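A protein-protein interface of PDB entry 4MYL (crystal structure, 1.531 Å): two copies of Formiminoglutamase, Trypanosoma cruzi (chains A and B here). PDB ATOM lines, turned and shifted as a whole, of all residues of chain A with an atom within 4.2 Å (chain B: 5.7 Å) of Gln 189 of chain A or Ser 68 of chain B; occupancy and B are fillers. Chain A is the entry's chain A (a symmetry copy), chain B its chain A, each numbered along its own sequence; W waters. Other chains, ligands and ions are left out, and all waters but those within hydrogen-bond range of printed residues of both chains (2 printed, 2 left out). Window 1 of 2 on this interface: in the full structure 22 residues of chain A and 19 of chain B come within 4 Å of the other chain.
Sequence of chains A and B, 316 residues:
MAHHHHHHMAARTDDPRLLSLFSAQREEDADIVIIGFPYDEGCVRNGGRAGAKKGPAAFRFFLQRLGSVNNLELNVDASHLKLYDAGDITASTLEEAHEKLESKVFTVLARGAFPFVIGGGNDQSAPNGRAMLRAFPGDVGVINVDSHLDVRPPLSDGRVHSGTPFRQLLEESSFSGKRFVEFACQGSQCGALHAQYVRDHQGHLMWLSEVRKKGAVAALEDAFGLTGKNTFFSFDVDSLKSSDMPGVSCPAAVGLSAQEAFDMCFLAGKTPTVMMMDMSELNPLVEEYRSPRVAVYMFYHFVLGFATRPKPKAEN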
ATOM      1  N   SER A 147      -9.011  -4.824  17.993  1.00  0.00           N
ATOM      2  CA  SER A 147      -8.326  -4.864  19.283  1.00  0.00           C
ATOM      3  C   SER A 147      -7.077  -3.970  19.300  1.00  0.00           C
ATOM      4  O   SER A 147      -6.633  -3.538  20.364  1.00  0.00           O
ATOM      5  CB  SER A 147      -7.920  -6.302  19.610  1.00  0.00           C
ATOM      6  OG  SER A 147      -7.123  -6.834  18.571  1.00  0.00           O
ATOM      7  N   HIS A 148      -6.521  -3.724  18.113  1.00  0.00           N
ATOM      8  CA  HIS A 148      -5.345  -2.863  17.908  1.00  0.00           C
ATOM      9  C   HIS A 148      -5.764  -1.524  17.318  1.00  0.00           C
ATOM     10  O   HIS A 148      -6.873  -1.393  16.799  1.00  0.00           O
ATOM     11  CB  HIS A 148      -4.334  -3.533  16.965  1.00  0.00           C
ATOM     12  CG  HIS A 148      -3.709  -4.770  17.533  1.00  0.00           C
ATOM     13  ND1 HIS A 148      -4.293  -6.016  17.433  1.00  0.00           N
ATOM     14  CD2 HIS A 148      -2.555  -4.951  18.215  1.00  0.00           C
ATOM     15  CE1 HIS A 148      -3.525  -6.912  18.026  1.00  0.00           C
ATOM     16  NE2 HIS A 148      -2.462  -6.294  18.503  1.00  0.00           N
ATOM     17  N   GLN A 186      -8.077  -2.749  22.777  1.00  0.00           N
ATOM     18  CA  GLN A 186      -7.702  -3.372  24.044  1.00  0.00           C
ATOM     19  C   GLN A 186      -6.392  -2.789  24.586  1.00  0.00           C
ATOM     20  O   GLN A 186      -5.370  -2.849  23.908  1.00  0.00           O
ATOM     21  CB  GLN A 186      -7.574  -4.885  23.851  1.00  0.00           C
ATOM     22  CG  GLN A 186      -8.886  -5.546  23.510  1.00  0.00           C
ATOM     23  CD  GLN A 186      -8.754  -7.044  23.307  1.00  0.00           C
ATOM     24  OE1 GLN A 186      -7.757  -7.651  23.694  1.00  0.00           O
ATOM     25  NE2 GLN A 186      -9.767  -7.646  22.699  1.00  0.00           N
ATOM     26  N   GLY A 187      -6.427  -2.244  25.801  1.00  0.00           N
ATOM     27  CA  GLY A 187      -5.263  -1.606  26.387  1.00  0.00           C
ATOM     28  C   GLY A 187      -4.049  -2.513  26.497  1.00  0.00           C
ATOM     29  O   GLY A 187      -2.914  -2.060  26.430  1.00  0.00           O
ATOM     30  N   SER A 188      -4.277  -3.808  26.657  1.00  0.00           N
ATOM     31  CA  SER A 188      -3.171  -4.762  26.803  1.00  0.00           C
ATOM     32  C   SER A 188      -2.401  -4.998  25.507  1.00  0.00           C
ATOM     33  O   SER A 188      -1.306  -5.541  25.534  1.00  0.00           O
ATOM     34  CB  SER A 188      -3.707  -6.107  27.277  1.00  0.00           C
ATOM     35  OG  SER A 188      -4.547  -6.641  26.273  1.00  0.00           O
ATOM     36  N   GLN A 189      -2.995  -4.616  24.376  1.00  0.00           N
ATOM     37  CA  GLN A 189      -2.436  -4.899  23.055  1.00  0.00           C
ATOM     38  C   GLN A 189      -1.991  -3.634  22.337  1.00  0.00           C
ATOM     39  O   GLN A 189      -1.349  -3.704  21.292  1.00  0.00           O
ATOM     40  CB  GLN A 189      -3.454  -5.639  22.177  1.00  0.00           C
ATOM     41  CG  GLN A 189      -3.973  -6.949  22.749  1.00  0.00           C
ATOM     42  CD  GLN A 189      -4.376  -7.913  21.658  1.00  0.00           C
ATOM     43  OE1 GLN A 189      -3.548  -8.299  20.834  1.00  0.00           O
ATOM     44  NE2 GLN A 189      -5.643  -8.304  21.638  1.00  0.00           N
ATOM     45  N   CYS A 190      -2.334  -2.484  22.907  1.00  0.00           N
ATOM     46  CA  CYS A 190      -2.109  -1.196  22.259  1.00  0.00           C
ATOM     47  C   CYS A 190      -1.053  -0.361  22.982  1.00  0.00           C
ATOM     48  O   CYS A 190      -1.170  -0.111  24.183  1.00  0.00           O
ATOM     49  CB  CYS A 190      -3.419  -0.411  22.193  1.00  0.00           C
ATOM     50  SG  CYS A 190      -4.671  -1.175  21.153  1.00  0.00           S
ATOM     51  N   GLY A 191      -0.033   0.075  22.247  1.00  0.00           N
ATOM     52  CA  GLY A 191       1.057   0.828  22.848  1.00  0.00           C
ATOM     53  C   GLY A 191       0.617   2.237  23.189  1.00  0.00           C
ATOM     54  O   GLY A 191      -0.237   2.784  22.497  1.00  0.00           O
ATOM     55  N   ASP B  15       6.777   0.141  21.777  1.00  0.00           N
ATOM     56  CA  ASP B  15       5.548  -0.427  22.311  1.00  0.00           C
ATOM     57  C   ASP B  15       6.020  -1.436  23.347  1.00  0.00           C
ATOM     58  O   ASP B  15       5.969  -2.639  23.115  1.00  0.00           O
ATOM     59  CB  ASP B  15       4.752  -1.113  21.187  1.00  0.00           C
ATOM     60  CG  ASP B  15       3.513  -1.862  21.693  1.00  0.00           C
ATOM     61  OD1 ASP B  15       3.144  -1.723  22.880  1.00  0.00           O
ATOM     62  OD2 ASP B  15       2.904  -2.599  20.887  1.00  0.00           O
ATOM     63  N   PRO B  16       6.531  -0.937  24.484  1.00  0.00           N
ATOM     64  CA  PRO B  16       7.182  -1.789  25.484  1.00  0.00           C
ATOM     65  C   PRO B  16       6.175  -2.706  26.146  1.00  0.00           C
ATOM     66  O   PRO B  16       5.061  -2.265  26.460  1.00  0.00           O
ATOM     67  CB  PRO B  16       7.720  -0.790  26.513  1.00  0.00           C
ATOM     68  CG  PRO B  16       7.705   0.530  25.829  1.00  0.00           C
ATOM     69  CD  PRO B  16       6.584   0.487  24.848  1.00  0.00           C
ATOM     70  N   ARG B  17       6.576  -3.953  26.369  1.00  0.00           N
ATOM     71  CA  ARG B  17       5.697  -4.942  26.972  1.00  0.00           C
ATOM     72  C   ARG B  17       6.330  -5.588  28.201  1.00  0.00           C
ATOM     73  O   ARG B  17       7.343  -5.118  28.693  1.00  0.00           O
ATOM     74  CB  ARG B  17       5.238  -5.967  25.929  1.00  0.00           C
ATOM     75  CG  ARG B  17       4.219  -5.379  24.947  1.00  0.00           C
ATOM     76  CD  ARG B  17       3.819  -6.374  23.872  1.00  0.00           C
ATOM     77  NE  ARG B  17       2.706  -5.888  23.045  1.00  0.00           N
ATOM     78  CZ  ARG B  17       2.032  -6.633  22.167  1.00  0.00           C
ATOM     79  NH1 ARG B  17       2.344  -7.916  21.979  1.00  0.00           N
ATOM     80  NH2 ARG B  17       1.034  -6.097  21.473  1.00  0.00           N
ATOM     81  N   LEU B  18       5.715  -6.645  28.713  1.00  0.00           N
ATOM     82  CA  LEU B  18       6.174  -7.243  29.958  1.00  0.00           C
ATOM     83  C   LEU B  18       7.666  -7.538  29.926  1.00  0.00           C
ATOM     84  O   LEU B  18       8.353  -7.367  30.929  1.00  0.00           O
ATOM     85  CB  LEU B  18       5.373  -8.518  30.290  1.00  0.00           C
ATOM     86  CG  LEU B  18       3.974  -8.342  30.901  1.00  0.00           C
ATOM     87  CD1 LEU B  18       3.220  -9.639  30.941  1.00  0.00           C
ATOM     88  CD2 LEU B  18       4.059  -7.755  32.304  1.00  0.00           C
ATOM     89  N   LEU B  66       3.812 -10.552  25.243  1.00  0.00           N
ATOM     90  CA  LEU B  66       2.530  -9.897  25.526  1.00  0.00           C
ATOM     91  C   LEU B  66       2.599  -8.825  26.610  1.00  0.00           C
ATOM     92  O   LEU B  66       3.494  -8.823  27.444  1.00  0.00           O
ATOM     93  CB  LEU B  66       1.482 -10.944  25.949  1.00  0.00           C
ATOM     94  CG  LEU B  66       1.257 -12.202  25.098  1.00  0.00           C
ATOM     95  CD1 LEU B  66       0.135 -13.049  25.688  1.00  0.00           C
ATOM     96  CD2 LEU B  66       0.922 -11.820  23.678  1.00  0.00           C
ATOM     97  N   GLY B  67       1.623  -7.924  26.602  1.00  0.00           N
ATOM     98  CA  GLY B  67       1.351  -7.063  27.746  1.00  0.00           C
ATOM     99  C   GLY B  67       1.888  -5.640  27.709  1.00  0.00           C
ATOM    100  O   GLY B  67       2.999  -5.399  28.166  1.00  0.00           O
ATOM    101  N   SER B  68       1.097  -4.692  27.206  1.00  0.00           N
ATOM    102  CA  SER B  68       1.542  -3.301  27.161  1.00  0.00           C
ATOM    103  C   SER B  68       1.877  -2.839  28.571  1.00  0.00           C
ATOM    104  O   SER B  68       1.037  -2.935  29.459  1.00  0.00           O
ATOM    105  CB  SER B  68       0.452  -2.393  26.586  1.00  0.00           C
ATOM    106  OG  SER B  68       0.008  -2.837  25.319  1.00  0.00           O
ATOM    107  N   VAL B  69       3.088  -2.327  28.785  1.00  0.00           N
ATOM    108  CA  VAL B  69       3.474  -1.879  30.131  1.00  0.00           C
ATOM    109  C   VAL B  69       2.727  -0.612  30.570  1.00  0.00           C
ATOM    110  O   VAL B  69       2.497  -0.404  31.752  1.00  0.00           O
ATOM    111  CB  VAL B  69       5.011  -1.690  30.307  1.00  0.00           C
ATOM    112  CG1 VAL B  69       5.733  -3.020  30.162  1.00  0.00           C
ATOM    113  CG2 VAL B  69       5.559  -0.656  29.337  1.00  0.00           C
ATOM    114  N   ASN B  70       2.354   0.238  29.620  1.00  0.00           N
ATOM    115  CA  ASN B  70       1.471   1.349  29.940  1.00  0.00           C
ATOM    116  C   ASN B  70       0.136   1.082  29.292  1.00  0.00           C
ATOM    117  O   ASN B  70       0.022   1.072  28.061  1.00  0.00           O
ATOM    118  CB  ASN B  70       2.046   2.677  29.456  1.00  0.00           C
ATOM    119  CG  ASN B  70       1.289   3.880  30.004  1.00  0.00           C
ATOM    120  OD1 ASN B  70       0.330   3.741  30.771  1.00  0.00           O
ATOM    121  ND2 ASN B  70       1.726   5.075  29.611  1.00  0.00           N
ATOM    122  N   ASN B  71      -0.865   0.836  30.120  1.00  0.00           N
ATOM    123  CA  ASN B  71      -2.172   0.421  29.628  1.00  0.00           C
ATOM    124  C   ASN B  71      -3.161   1.571  29.768  1.00  0.00           C
ATOM    125  O   ASN B  71      -3.522   1.964  30.876  1.00  0.00           O
ATOM    126  CB  ASN B  71      -2.636  -0.808  30.405  1.00  0.00           C
ATOM    127  CG  ASN B  71      -3.975  -1.317  29.944  1.00  0.00           C
ATOM    128  OD1 ASN B  71      -4.902  -0.539  29.700  1.00  0.00           O
ATOM    129  ND2 ASN B  71      -4.101  -2.640  29.848  1.00  0.00           N
ATOM    130  N   ARG B 293      -1.709 -17.861  26.543  1.00  0.00           N
ATOM    131  CA  ARG B 293      -1.943 -16.414  26.430  1.00  0.00           C
ATOM    132  C   ARG B 293      -2.836 -15.903  27.573  1.00  0.00           C
ATOM    133  O   ARG B 293      -2.555 -14.891  28.200  1.00  0.00           O
ATOM    134  CB  ARG B 293      -2.539 -16.051  25.065  1.00  0.00           C
ATOM    135  CG  ARG B 293      -1.566 -16.288  23.901  1.00  0.00           C
ATOM    136  CD  ARG B 293      -2.154 -15.901  22.529  1.00  0.00           C
ATOM    137  NE  ARG B 293      -2.417 -14.470  22.447  1.00  0.00           N
ATOM    138  CZ  ARG B 293      -1.713 -13.613  21.711  1.00  0.00           C
ATOM    139  NH1 ARG B 293      -0.698 -14.044  20.976  1.00  0.00           N
ATOM    140  NH2 ARG B 293      -2.032 -12.326  21.705  1.00  0.00           N
ATOM    141  N   TYR B 297      -1.810 -13.186  30.356  1.00  0.00           N
ATOM    142  CA  TYR B 297      -2.662 -12.022  30.581  1.00  0.00           C
ATOM    143  C   TYR B 297      -3.187 -11.932  32.017  1.00  0.00           C
ATOM    144  O   TYR B 297      -3.372 -10.843  32.554  1.00  0.00           O
ATOM    145  CB  TYR B 297      -3.799 -11.973  29.558  1.00  0.00           C
ATOM    146  CG  TYR B 297      -3.364 -11.445  28.207  1.00  0.00           C
ATOM    147  CD1 TYR B 297      -2.622 -10.271  28.105  1.00  0.00           C
ATOM    148  CD2 TYR B 297      -3.710 -12.109  27.031  1.00  0.00           C
ATOM    149  CE1 TYR B 297      -2.224  -9.775  26.865  1.00  0.00           C
ATOM    150  CE2 TYR B 297      -3.316 -11.621  25.782  1.00  0.00           C
ATOM    151  CZ  TYR B 297      -2.575 -10.454  25.714  1.00  0.00           C
ATOM    152  OH  TYR B 297      -2.185  -9.961  24.489  1.00  0.00           O
ATOM    153  N   TYR B 300      -0.221 -10.609  33.784  1.00  0.00           N
ATOM    154  CA  TYR B 300      -0.148  -9.217  33.342  1.00  0.00           C
ATOM    155  C   TYR B 300      -1.068  -8.297  34.159  1.00  0.00           C
ATOM    156  O   TYR B 300      -0.656  -7.238  34.642  1.00  0.00           O
ATOM    157  CB  TYR B 300      -0.505  -9.164  31.854  1.00  0.00           C
ATOM    158  CG  TYR B 300      -0.723  -7.779  31.300  1.00  0.00           C
ATOM    159  CD1 TYR B 300       0.337  -6.896  31.147  1.00  0.00           C
ATOM    160  CD2 TYR B 300      -1.983  -7.364  30.906  1.00  0.00           C
ATOM    161  CE1 TYR B 300       0.139  -5.628  30.629  1.00  0.00           C
ATOM    162  CE2 TYR B 300      -2.191  -6.103  30.389  1.00  0.00           C
ATOM    163  CZ  TYR B 300      -1.125  -5.239  30.247  1.00  0.00           C
ATOM    164  OH  TYR B 300      -1.324  -3.977  29.724  1.00  0.00           O
ATOM    165  N   LEU B 304      -0.171  -5.170  36.654  1.00  0.00           N
ATOM    166  CA  LEU B 304      -0.803  -3.853  36.597  1.00  0.00           C
ATOM    167  C   LEU B 304      -1.400  -3.424  37.942  1.00  0.00           C
ATOM    168  O   LEU B 304      -1.189  -2.292  38.385  1.00  0.00           O
ATOM    169  CB  LEU B 304      -1.873  -3.816  35.513  1.00  0.00           C
ATOM    170  CG  LEU B 304      -1.379  -3.922  34.073  1.00  0.00           C
ATOM    171  CD1 LEU B 304      -2.555  -3.759  33.132  1.00  0.00           C
ATOM    172  CD2 LEU B 304      -0.333  -2.878  33.772  1.00  0.00           C
HETATM  173  O   HOH W   1       1.461  -3.570  23.066  1.00  0.00           O
HETATM  174  O   HOH W   2      -0.316  -7.863  24.474  1.00  0.00           O
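No position is printed for both chains.
Of the 12 pairs that touch across the chains among the printed residues, none has its exchanged pair printed and touching as well.
Water W1 lies within hydrogen-bond range of the side-chain carboxylate of Asp 15 of chain B (2.5 Å), the guanidinium group of Arg 17 of chain B (2.6 Å), the side-chain hydroxyl of Ser 68 of chain B (2.8 Å) and the backbone carbonyl oxygen of Gln 189 of chain A (3.3 Å).
Water W2 lies within hydrogen-bond range of O of Ser 188 of chain A (2.7 Å), OH of Tyr 297 of chain B (2.8 Å) and N of Gly 67 of chain B (2.9 Å).
Of the 8 printed residues of chain A, 5 touch a printed residue of chain B.
Of the 14 printed residues of chain B, 7 touch a printed residue of chain A.
Printed residues of chain B that touch a printed residue of chain A: Asp 15, Arg 17, Gly 67, Ser 68, Asn 71, Tyr 297 and Tyr 300.
Hydrophobic or aromatic side chains of chain B within 4 Å of the printed part of chain A: Tyr 297 and Tyr 300.
Among the printed residues, 12 pairs touch across the chains.
Among the printed residues, no Asp or Glu carboxylate lies within 4 Å of a Lys or Arg side-chain nitrogen of the other chain.
N of Leu 18 of chain B sits at hydrogen-bond distance from O of Gly 67 of chain B, at 3.0 Å.
The backbone carbonyl oxygen of Ser 68 of chain B lies within hydrogen-bond range of the side-chain hydroxyl of Tyr 300 of chain B (2.6 Å).
The side-chain sulfur of Cys 190 of chain A lies within hydrogen-bond range of the backbone carbonyl oxygen of Ser 147 of chain A (3.2 Å).
OE1 of Gln 189 of chain A lies close to NE2 of His 148 of chain A, at 3.3 Å.
The side-chain amide nitrogen (NE2) of Gln 189 of chain A lies within hydrogen-bond range of the side-chain amide oxygen (OE1) of Gln 186 of chain A (3.0 Å).
O of Gln 186 of chain A is in hydrogen-bond range of SG of Cys 190 of chain A, 3.3 Å away.
Among the printed residues, merely in contact across the chains: Gly 191 of chain A with Asp 15 of chain B, Gly 187 of chain A with Asn 71 of chain B, Ser 188 of chain A with Tyr 300 of chain B, Gln 189 of chain A with Ser 68 of chain B, Ser 188 of chain A with Gly 67 of chain B, Gln 189 of chain A with Tyr 297 of chain B and Ser 188 of chain A with Tyr 297 of chain B.
NH2 of Arg 17 of chain B lies within hydrogen-bond range of O of Gln 189 of chain A.
The backbone carbonyl oxygen (O) of Gly 187 of chain A lies within hydrogen-bond range of the side-chain hydroxyl (OG) of Ser 68 of chain B (3.2 Å).
The backbone carbonyl oxygen (O) of Ser 188 of chain A sits at hydrogen-bond distance from the side-chain hydroxyl (OG) of Ser 68 of chain B (3.0 Å).
The backbone carbonyl oxygen (O) of Cys 190 of chain A is in hydrogen-bond range of the side-chain hydroxyl (OG) of Ser 68 of chain B (3.2 Å).
The side-chain amide nitrogen (ND2) of Asn 71 of chain B lies close to the backbone NH (N) of Ser 188 of chain A, at 3.4 Å.
Of chain B, only Arg 17, Ser 68 and Tyr 297 come within 4 Å of Gln 189 of chain A.
Of chain A, only Gly 187 (3.2 Å), Ser 188 (3.0 Å), Gln 189 (3.6 Å) and Cys 190 (3.2 Å) come within 4 Å of Ser 68 of chain B.
Of the printed residues of chain A, Asn 71 of chain B touches Gly 187 and Ser 188.
Of the printed residues of chain B, Ser 188 of chain A touches Gly 67, Ser 68, Asn 71, Tyr 297 and Tyr 300.
Of the printed residues of chain A, Tyr 297 of chain B touches Ser 188 and Gln 189.
Of the printed residues of chain B, Gly 191 of chain A touches Asp 15 (3.3 Å).
Of the printed residues of chain A, Arg 17 of chain B touches Gln 189 (3.4 Å).
Arg 293 of chain B touches none of the printed residues of chain A.
Leu 304 of chain B touches none of the printed residues of chain A.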
